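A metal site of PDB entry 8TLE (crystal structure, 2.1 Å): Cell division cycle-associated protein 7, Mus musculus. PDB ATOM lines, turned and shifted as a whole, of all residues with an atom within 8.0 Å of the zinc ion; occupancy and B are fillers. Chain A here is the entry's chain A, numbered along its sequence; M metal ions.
The side-chain sulfur of Cys 96 sits close to the side-chain amide nitrogen of Asn 59 (3.1 Å).
SG of Cys 96 lies close to NH2 of Arg 66 (3.5 Å).
The side-chain sulfur of Cys 57 sits close to the backbone NH of Asn 59 (3.5 Å).
NE2 of His 10 sits at hydrogen-bond distance from O of Cys 57.
SG of Cys 62 lies close to NE of Arg 66 (3.6 Å).
O of Cys 62 is in hydrogen-bond range of ND1 of His 10 (3.4 Å).
Of the 22 residues printed, 4 come within 4 Å of the zinc ion.
The nearest printed residue that does not touch the zinc ion is Asn 59 (4.3 Å).
The zinc ion is bound by SG of Cys 93 (2.3 Å), SG of Cys 96 (2.3 Å), SG of Cys 57 (2.3 Å) and SG of Cys 62 (2.3 Å).
The zinc ion has four donor atoms within binding distance.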
ATOM      1  N   HIS A  10      -2.578 -30.710  24.643  1.00  0.00           N
ATOM      2  CA  HIS A  10      -2.921 -29.332  24.374  1.00  0.00           C
ATOM      3  C   HIS A  10      -2.947 -29.103  22.863  1.00  0.00           C
ATOM      4  O   HIS A  10      -1.938 -29.300  22.183  1.00  0.00           O
ATOM      5  CB  HIS A  10      -1.918 -28.384  25.043  1.00  0.00           C
ATOM      6  CG  HIS A  10      -2.085 -26.951  24.645  1.00  0.00           C
ATOM      7  ND1 HIS A  10      -1.080 -26.234  24.022  1.00  0.00           N
ATOM      8  CD2 HIS A  10      -3.122 -26.095  24.784  1.00  0.00           C
ATOM      9  CE1 HIS A  10      -1.500 -25.005  23.800  1.00  0.00           C
ATOM     10  NE2 HIS A  10      -2.737 -24.892  24.244  1.00  0.00           N
ATOM     11  N   ASN A  56      -8.280 -20.724  25.099  1.00  0.00           N
ATOM     12  CA  ASN A  56      -7.323 -21.643  24.482  1.00  0.00           C
ATOM     13  C   ASN A  56      -5.994 -20.936  24.354  1.00  0.00           C
ATOM     14  O   ASN A  56      -5.885 -19.944  23.617  1.00  0.00           O
ATOM     15  CB  ASN A  56      -7.823 -22.125  23.112  1.00  0.00           C
ATOM     16  CG  ASN A  56      -6.782 -22.911  22.361  1.00  0.00           C
ATOM     17  OD1 ASN A  56      -6.021 -22.360  21.561  1.00  0.00           O
ATOM     18  ND2 ASN A  56      -6.731 -24.216  22.599  1.00  0.00           N
ATOM     19  N   CYS A  57      -4.981 -21.441  25.050  1.00  0.00           N
ATOM     20  CA  CYS A  57      -3.654 -20.830  24.993  1.00  0.00           C
ATOM     21  C   CYS A  57      -2.994 -21.136  23.661  1.00  0.00           C
ATOM     22  O   CYS A  57      -2.939 -22.294  23.232  1.00  0.00           O
ATOM     23  CB  CYS A  57      -2.790 -21.333  26.140  1.00  0.00           C
ATOM     24  SG  CYS A  57      -1.182 -20.522  26.268  1.00  0.00           S
ATOM     25  N   ARG A  58      -2.503 -20.091  22.991  1.00  0.00           N
ATOM     26  CA  ARG A  58      -1.854 -20.239  21.699  1.00  0.00           C
ATOM     27  C   ARG A  58      -0.337 -20.434  21.803  1.00  0.00           C
ATOM     28  O   ARG A  58       0.332 -20.506  20.772  1.00  0.00           O
ATOM     29  CB  ARG A  58      -2.139 -19.022  20.815  1.00  0.00           C
ATOM     30  CG  ARG A  58      -3.422 -19.134  19.998  1.00  0.00           C
ATOM     31  CD  ARG A  58      -4.651 -18.797  20.825  1.00  0.00           C
ATOM     32  NE  ARG A  58      -5.875 -18.926  20.042  1.00  0.00           N
ATOM     33  CZ  ARG A  58      -7.081 -18.553  20.468  1.00  0.00           C
ATOM     34  NH1 ARG A  58      -7.255 -18.010  21.654  1.00  0.00           N
ATOM     35  NH2 ARG A  58      -8.128 -18.731  19.668  1.00  0.00           N
ATOM     36  N   ASN A  59       0.197 -20.514  23.013  1.00  0.00           N
ATOM     37  CA  ASN A  59       1.626 -20.754  23.178  1.00  0.00           C
ATOM     38  C   ASN A  59       1.938 -22.210  22.839  1.00  0.00           C
ATOM     39  O   ASN A  59       1.380 -23.114  23.474  1.00  0.00           O
ATOM     40  CB  ASN A  59       2.063 -20.435  24.605  1.00  0.00           C
ATOM     41  CG  ASN A  59       3.535 -20.691  24.853  1.00  0.00           C
ATOM     42  OD1 ASN A  59       4.335 -20.676  23.913  1.00  0.00           O
ATOM     43  ND2 ASN A  59       3.898 -20.931  26.101  1.00  0.00           N
ATOM     44  N   PRO A  60       2.809 -22.477  21.866  1.00  0.00           N
ATOM     45  CA  PRO A  60       3.161 -23.874  21.565  1.00  0.00           C
ATOM     46  C   PRO A  60       3.817 -24.591  22.727  1.00  0.00           C
ATOM     47  O   PRO A  60       3.651 -25.814  22.862  1.00  0.00           O
ATOM     48  CB  PRO A  60       4.118 -23.746  20.366  1.00  0.00           C
ATOM     49  CG  PRO A  60       3.792 -22.418  19.757  1.00  0.00           C
ATOM     50  CD  PRO A  60       3.419 -21.540  20.912  1.00  0.00           C
ATOM     51  N   ASP A  61       4.556 -23.879  23.571  1.00  0.00           N
ATOM     52  CA  ASP A  61       5.227 -24.492  24.711  1.00  0.00           C
ATOM     53  C   ASP A  61       4.278 -24.835  25.855  1.00  0.00           C
ATOM     54  O   ASP A  61       4.676 -25.559  26.772  1.00  0.00           O
ATOM     55  CB  ASP A  61       6.333 -23.557  25.223  1.00  0.00           C
ATOM     56  CG  ASP A  61       7.358 -23.237  24.158  1.00  0.00           C
ATOM     57  OD1 ASP A  61       7.628 -24.117  23.306  1.00  0.00           O
ATOM     58  OD2 ASP A  61       7.899 -22.113  24.177  1.00  0.00           O
ATOM     59  N   CYS A  62       3.037 -24.344  25.820  1.00  0.00           N
ATOM     60  CA  CYS A  62       2.083 -24.674  26.858  1.00  0.00           C
ATOM     61  C   CYS A  62       1.661 -26.137  26.741  1.00  0.00           C
ATOM     62  O   CYS A  62       1.791 -26.775  25.689  1.00  0.00           O
ATOM     63  CB  CYS A  62       0.857 -23.763  26.766  1.00  0.00           C
ATOM     64  SG  CYS A  62      -0.208 -23.770  28.234  1.00  0.00           S
ATOM     65  N   TRP A  63       1.167 -26.679  27.853  1.00  0.00           N
ATOM     66  CA  TRP A  63       0.765 -28.081  27.886  1.00  0.00           C
ATOM     67  C   TRP A  63      -0.399 -28.247  28.856  1.00  0.00           C
ATOM     68  O   TRP A  63      -0.627 -27.408  29.731  1.00  0.00           O
ATOM     69  CB  TRP A  63       1.932 -28.984  28.306  1.00  0.00           C
ATOM     70  CG  TRP A  63       2.296 -28.862  29.758  1.00  0.00           C
ATOM     71  CD1 TRP A  63       1.871 -29.658  30.779  1.00  0.00           C
ATOM     72  CD2 TRP A  63       3.165 -27.886  30.343  1.00  0.00           C
ATOM     73  NE1 TRP A  63       2.416 -29.239  31.963  1.00  0.00           N
ATOM     74  CE2 TRP A  63       3.215 -28.149  31.723  1.00  0.00           C
ATOM     75  CE3 TRP A  63       3.909 -26.818  29.836  1.00  0.00           C
ATOM     76  CZ2 TRP A  63       3.978 -27.382  32.609  1.00  0.00           C
ATOM     77  CZ3 TRP A  63       4.657 -26.058  30.705  1.00  0.00           C
ATOM     78  CH2 TRP A  63       4.690 -26.344  32.075  1.00  0.00           C
ATOM     79  N   GLY A  64      -1.126 -29.338  28.677  1.00  0.00           N
ATOM     80  CA  GLY A  64      -2.231 -29.637  29.564  1.00  0.00           C
ATOM     81  C   GLY A  64      -3.385 -28.651  29.426  1.00  0.00           C
ATOM     82  O   GLY A  64      -3.634 -28.081  28.360  1.00  0.00           O
ATOM     83  N   ILE A  65      -4.089 -28.447  30.536  1.00  0.00           N
ATOM     84  CA  ILE A  65      -5.253 -27.572  30.570  1.00  0.00           C
ATOM     85  C   ILE A  65      -4.992 -26.314  31.380  1.00  0.00           C
ATOM     86  O   ILE A  65      -5.937 -25.595  31.734  1.00  0.00           O
ATOM     87  CB  ILE A  65      -6.483 -28.316  31.112  1.00  0.00           C
ATOM     88  CG1 ILE A  65      -6.262 -28.709  32.570  1.00  0.00           C
ATOM     89  CG2 ILE A  65      -6.779 -29.542  30.257  1.00  0.00           C
ATOM     90  CD1 ILE A  65      -7.486 -29.279  33.235  1.00  0.00           C
ATOM     91  N   ARG A  66      -3.734 -26.023  31.701  1.00  0.00           N
ATOM     92  CA  ARG A  66      -3.429 -24.825  32.488  1.00  0.00           C
ATOM     93  C   ARG A  66      -3.740 -23.544  31.731  1.00  0.00           C
ATOM     94  O   ARG A  66      -3.761 -22.471  32.350  1.00  0.00           O
ATOM     95  CB  ARG A  66      -1.969 -24.838  32.935  1.00  0.00           C
ATOM     96  CG  ARG A  66      -0.958 -24.592  31.825  1.00  0.00           C
ATOM     97  CD  ARG A  66       0.448 -24.525  32.407  1.00  0.00           C
ATOM     98  NE  ARG A  66       1.385 -23.866  31.503  1.00  0.00           N
ATOM     99  CZ  ARG A  66       2.608 -23.484  31.849  1.00  0.00           C
ATOM    100  NH1 ARG A  66       3.071 -23.678  33.074  1.00  0.00           N
ATOM    101  NH2 ARG A  66       3.379 -22.881  30.949  1.00  0.00           N
ATOM    102  N   GLY A  67      -3.960 -23.623  30.417  1.00  0.00           N
ATOM    103  CA  GLY A  67      -4.351 -22.490  29.620  1.00  0.00           C
ATOM    104  C   GLY A  67      -5.844 -22.286  29.460  1.00  0.00           C
ATOM    105  O   GLY A  67      -6.259 -21.397  28.721  1.00  0.00           O
ATOM    106  N   GLN A  68      -6.656 -23.089  30.147  1.00  0.00           N
ATOM    107  CA  GLN A  68      -8.114 -23.019  30.026  1.00  0.00           C
ATOM    108  C   GLN A  68      -8.674 -22.208  31.186  1.00  0.00           C
ATOM    109  O   GLN A  68      -8.532 -22.607  32.352  1.00  0.00           O
ATOM    110  CB  GLN A  68      -8.719 -24.418  29.992  1.00  0.00           C
ATOM    111  CG  GLN A  68      -8.220 -25.291  28.863  1.00  0.00           C
ATOM    112  CD  GLN A  68      -8.790 -26.700  28.911  1.00  0.00           C
ATOM    113  OE1 GLN A  68      -9.553 -27.039  29.819  1.00  0.00           O
ATOM    114  NE2 GLN A  68      -8.410 -27.529  27.953  1.00  0.00           N
ATOM    115  N   PHE A  69      -9.313 -21.085  30.874  1.00  0.00           N
ATOM    116  CA  PHE A  69      -9.917 -20.218  31.866  1.00  0.00           C
ATOM    117  C   PHE A  69     -11.358 -19.920  31.477  1.00  0.00           C
ATOM    118  O   PHE A  69     -11.646 -19.653  30.310  1.00  0.00           O
ATOM    119  CB  PHE A  69      -9.137 -18.906  32.022  1.00  0.00           C
ATOM    120  CG  PHE A  69      -7.799 -19.075  32.683  1.00  0.00           C
ATOM    121  CD1 PHE A  69      -6.715 -19.578  31.986  1.00  0.00           C
ATOM    122  CD2 PHE A  69      -7.627 -18.739  34.019  1.00  0.00           C
ATOM    123  CE1 PHE A  69      -5.489 -19.736  32.597  1.00  0.00           C
ATOM    124  CE2 PHE A  69      -6.407 -18.886  34.643  1.00  0.00           C
ATOM    125  CZ  PHE A  69      -5.334 -19.388  33.932  1.00  0.00           C
ATOM    126  N   TRP A  91      -2.629 -14.752  22.165  1.00  0.00           N
ATOM    127  CA  TRP A  91      -2.989 -14.771  23.581  1.00  0.00           C
ATOM    128  C   TRP A  91      -2.261 -15.896  24.302  1.00  0.00           C
ATOM    129  O   TRP A  91      -2.271 -17.042  23.859  1.00  0.00           O
ATOM    130  CB  TRP A  91      -4.498 -14.924  23.740  1.00  0.00           C
ATOM    131  CG  TRP A  91      -4.967 -14.805  25.161  1.00  0.00           C
ATOM    132  CD1 TRP A  91      -5.269 -13.650  25.831  1.00  0.00           C
ATOM    133  CD2 TRP A  91      -5.197 -15.873  26.080  1.00  0.00           C
ATOM    134  NE1 TRP A  91      -5.677 -13.938  27.109  1.00  0.00           N
ATOM    135  CE2 TRP A  91      -5.631 -15.290  27.290  1.00  0.00           C
ATOM    136  CE3 TRP A  91      -5.065 -17.257  25.999  1.00  0.00           C
ATOM    137  CZ2 TRP A  91      -5.949 -16.064  28.412  1.00  0.00           C
ATOM    138  CZ3 TRP A  91      -5.375 -18.021  27.115  1.00  0.00           C
ATOM    139  CH2 TRP A  91      -5.804 -17.417  28.300  1.00  0.00           C
ATOM    140  N   HIS A  92      -1.642 -15.552  25.422  1.00  0.00           N
ATOM    141  CA  HIS A  92      -0.989 -16.524  26.292  1.00  0.00           C
ATOM    142  C   HIS A  92      -1.749 -16.610  27.610  1.00  0.00           C
ATOM    143  O   HIS A  92      -2.309 -15.623  28.099  1.00  0.00           O
ATOM    144  CB  HIS A  92       0.464 -16.127  26.567  1.00  0.00           C
ATOM    145  CG  HIS A  92       1.398 -16.412  25.424  1.00  0.00           C
ATOM    146  ND1 HIS A  92       0.963 -16.954  24.228  1.00  0.00           N
ATOM    147  CD2 HIS A  92       2.728 -16.227  25.298  1.00  0.00           C
ATOM    148  CE1 HIS A  92       1.995 -17.084  23.422  1.00  0.00           C
ATOM    149  NE2 HIS A  92       3.081 -16.654  24.042  1.00  0.00           N
ATOM    150  N   CYS A  93      -1.766 -17.815  28.188  1.00  0.00           N
ATOM    151  CA  CYS A  93      -2.417 -17.991  29.481  1.00  0.00           C
ATOM    152  C   CYS A  93      -1.571 -17.341  30.584  1.00  0.00           C
ATOM    153  O   CYS A  93      -0.354 -17.195  30.427  1.00  0.00           O
ATOM    154  CB  CYS A  93      -2.624 -19.470  29.783  1.00  0.00           C
ATOM    155  SG  CYS A  93      -1.109 -20.433  29.975  1.00  0.00           S
ATOM    156  N   PRO A  94      -2.195 -16.945  31.692  1.00  0.00           N
ATOM    157  CA  PRO A  94      -1.435 -16.358  32.809  1.00  0.00           C
ATOM    158  C   PRO A  94      -0.340 -17.280  33.322  1.00  0.00           C
ATOM    159  O   PRO A  94       0.739 -16.786  33.700  1.00  0.00           O
ATOM    160  CB  PRO A  94      -2.516 -16.114  33.867  1.00  0.00           C
ATOM    161  CG  PRO A  94      -3.754 -15.891  33.077  1.00  0.00           C
ATOM    162  CD  PRO A  94      -3.646 -16.796  31.873  1.00  0.00           C
ATOM    163  N   PRO A  95      -0.541 -18.611  33.376  1.00  0.00           N
ATOM    164  CA  PRO A  95       0.601 -19.472  33.715  1.00  0.00           C
ATOM    165  C   PRO A  95       1.776 -19.323  32.765  1.00  0.00           C
ATOM    166  O   PRO A  95       2.936 -19.370  33.205  1.00  0.00           O
ATOM    167  CB  PRO A  95      -0.010 -20.881  33.656  1.00  0.00           C
ATOM    168  CG  PRO A  95      -1.408 -20.674  34.026  1.00  0.00           C
ATOM    169  CD  PRO A  95      -1.804 -19.376  33.390  1.00  0.00           C
ATOM    170  N   CYS A  96       1.532 -19.145  31.469  1.00  0.00           N
ATOM    171  CA  CYS A  96       2.626 -18.918  30.528  1.00  0.00           C
ATOM    172  C   CYS A  96       3.268 -17.550  30.746  1.00  0.00           C
ATOM    173  O   CYS A  96       4.491 -17.409  30.621  1.00  0.00           O
ATOM    174  CB  CYS A  96       2.125 -19.055  29.088  1.00  0.00           C
ATOM    175  SG  CYS A  96       1.918 -20.768  28.536  1.00  0.00           S
ATOM    176  N   ARG A  97       2.469 -16.549  31.086  1.00  0.00           N
ATOM    177  CA  ARG A  97       2.983 -15.212  31.367  1.00  0.00           C
ATOM    178  C   ARG A  97       3.572 -15.079  32.766  1.00  0.00           C
ATOM    179  O   ARG A  97       4.115 -14.018  33.090  1.00  0.00           O
ATOM    180  CB  ARG A  97       1.871 -14.176  31.168  1.00  0.00           C
ATOM    181  CG  ARG A  97       1.535 -13.888  29.715  1.00  0.00           C
ATOM    182  CD  ARG A  97       0.368 -12.917  29.602  1.00  0.00           C
ATOM    183  NE  ARG A  97      -0.910 -13.551  29.892  1.00  0.00           N
ATOM    184  CZ  ARG A  97      -2.084 -12.936  29.854  1.00  0.00           C
ATOM    185  NH1 ARG A  97      -2.168 -11.648  29.559  1.00  0.00           N
ATOM    186  NH2 ARG A  97      -3.185 -13.621  30.127  1.00  0.00           N
HETATM  187 ZN    ZN M   1      -0.219 -21.431  28.151  1.00  0.00          ZN
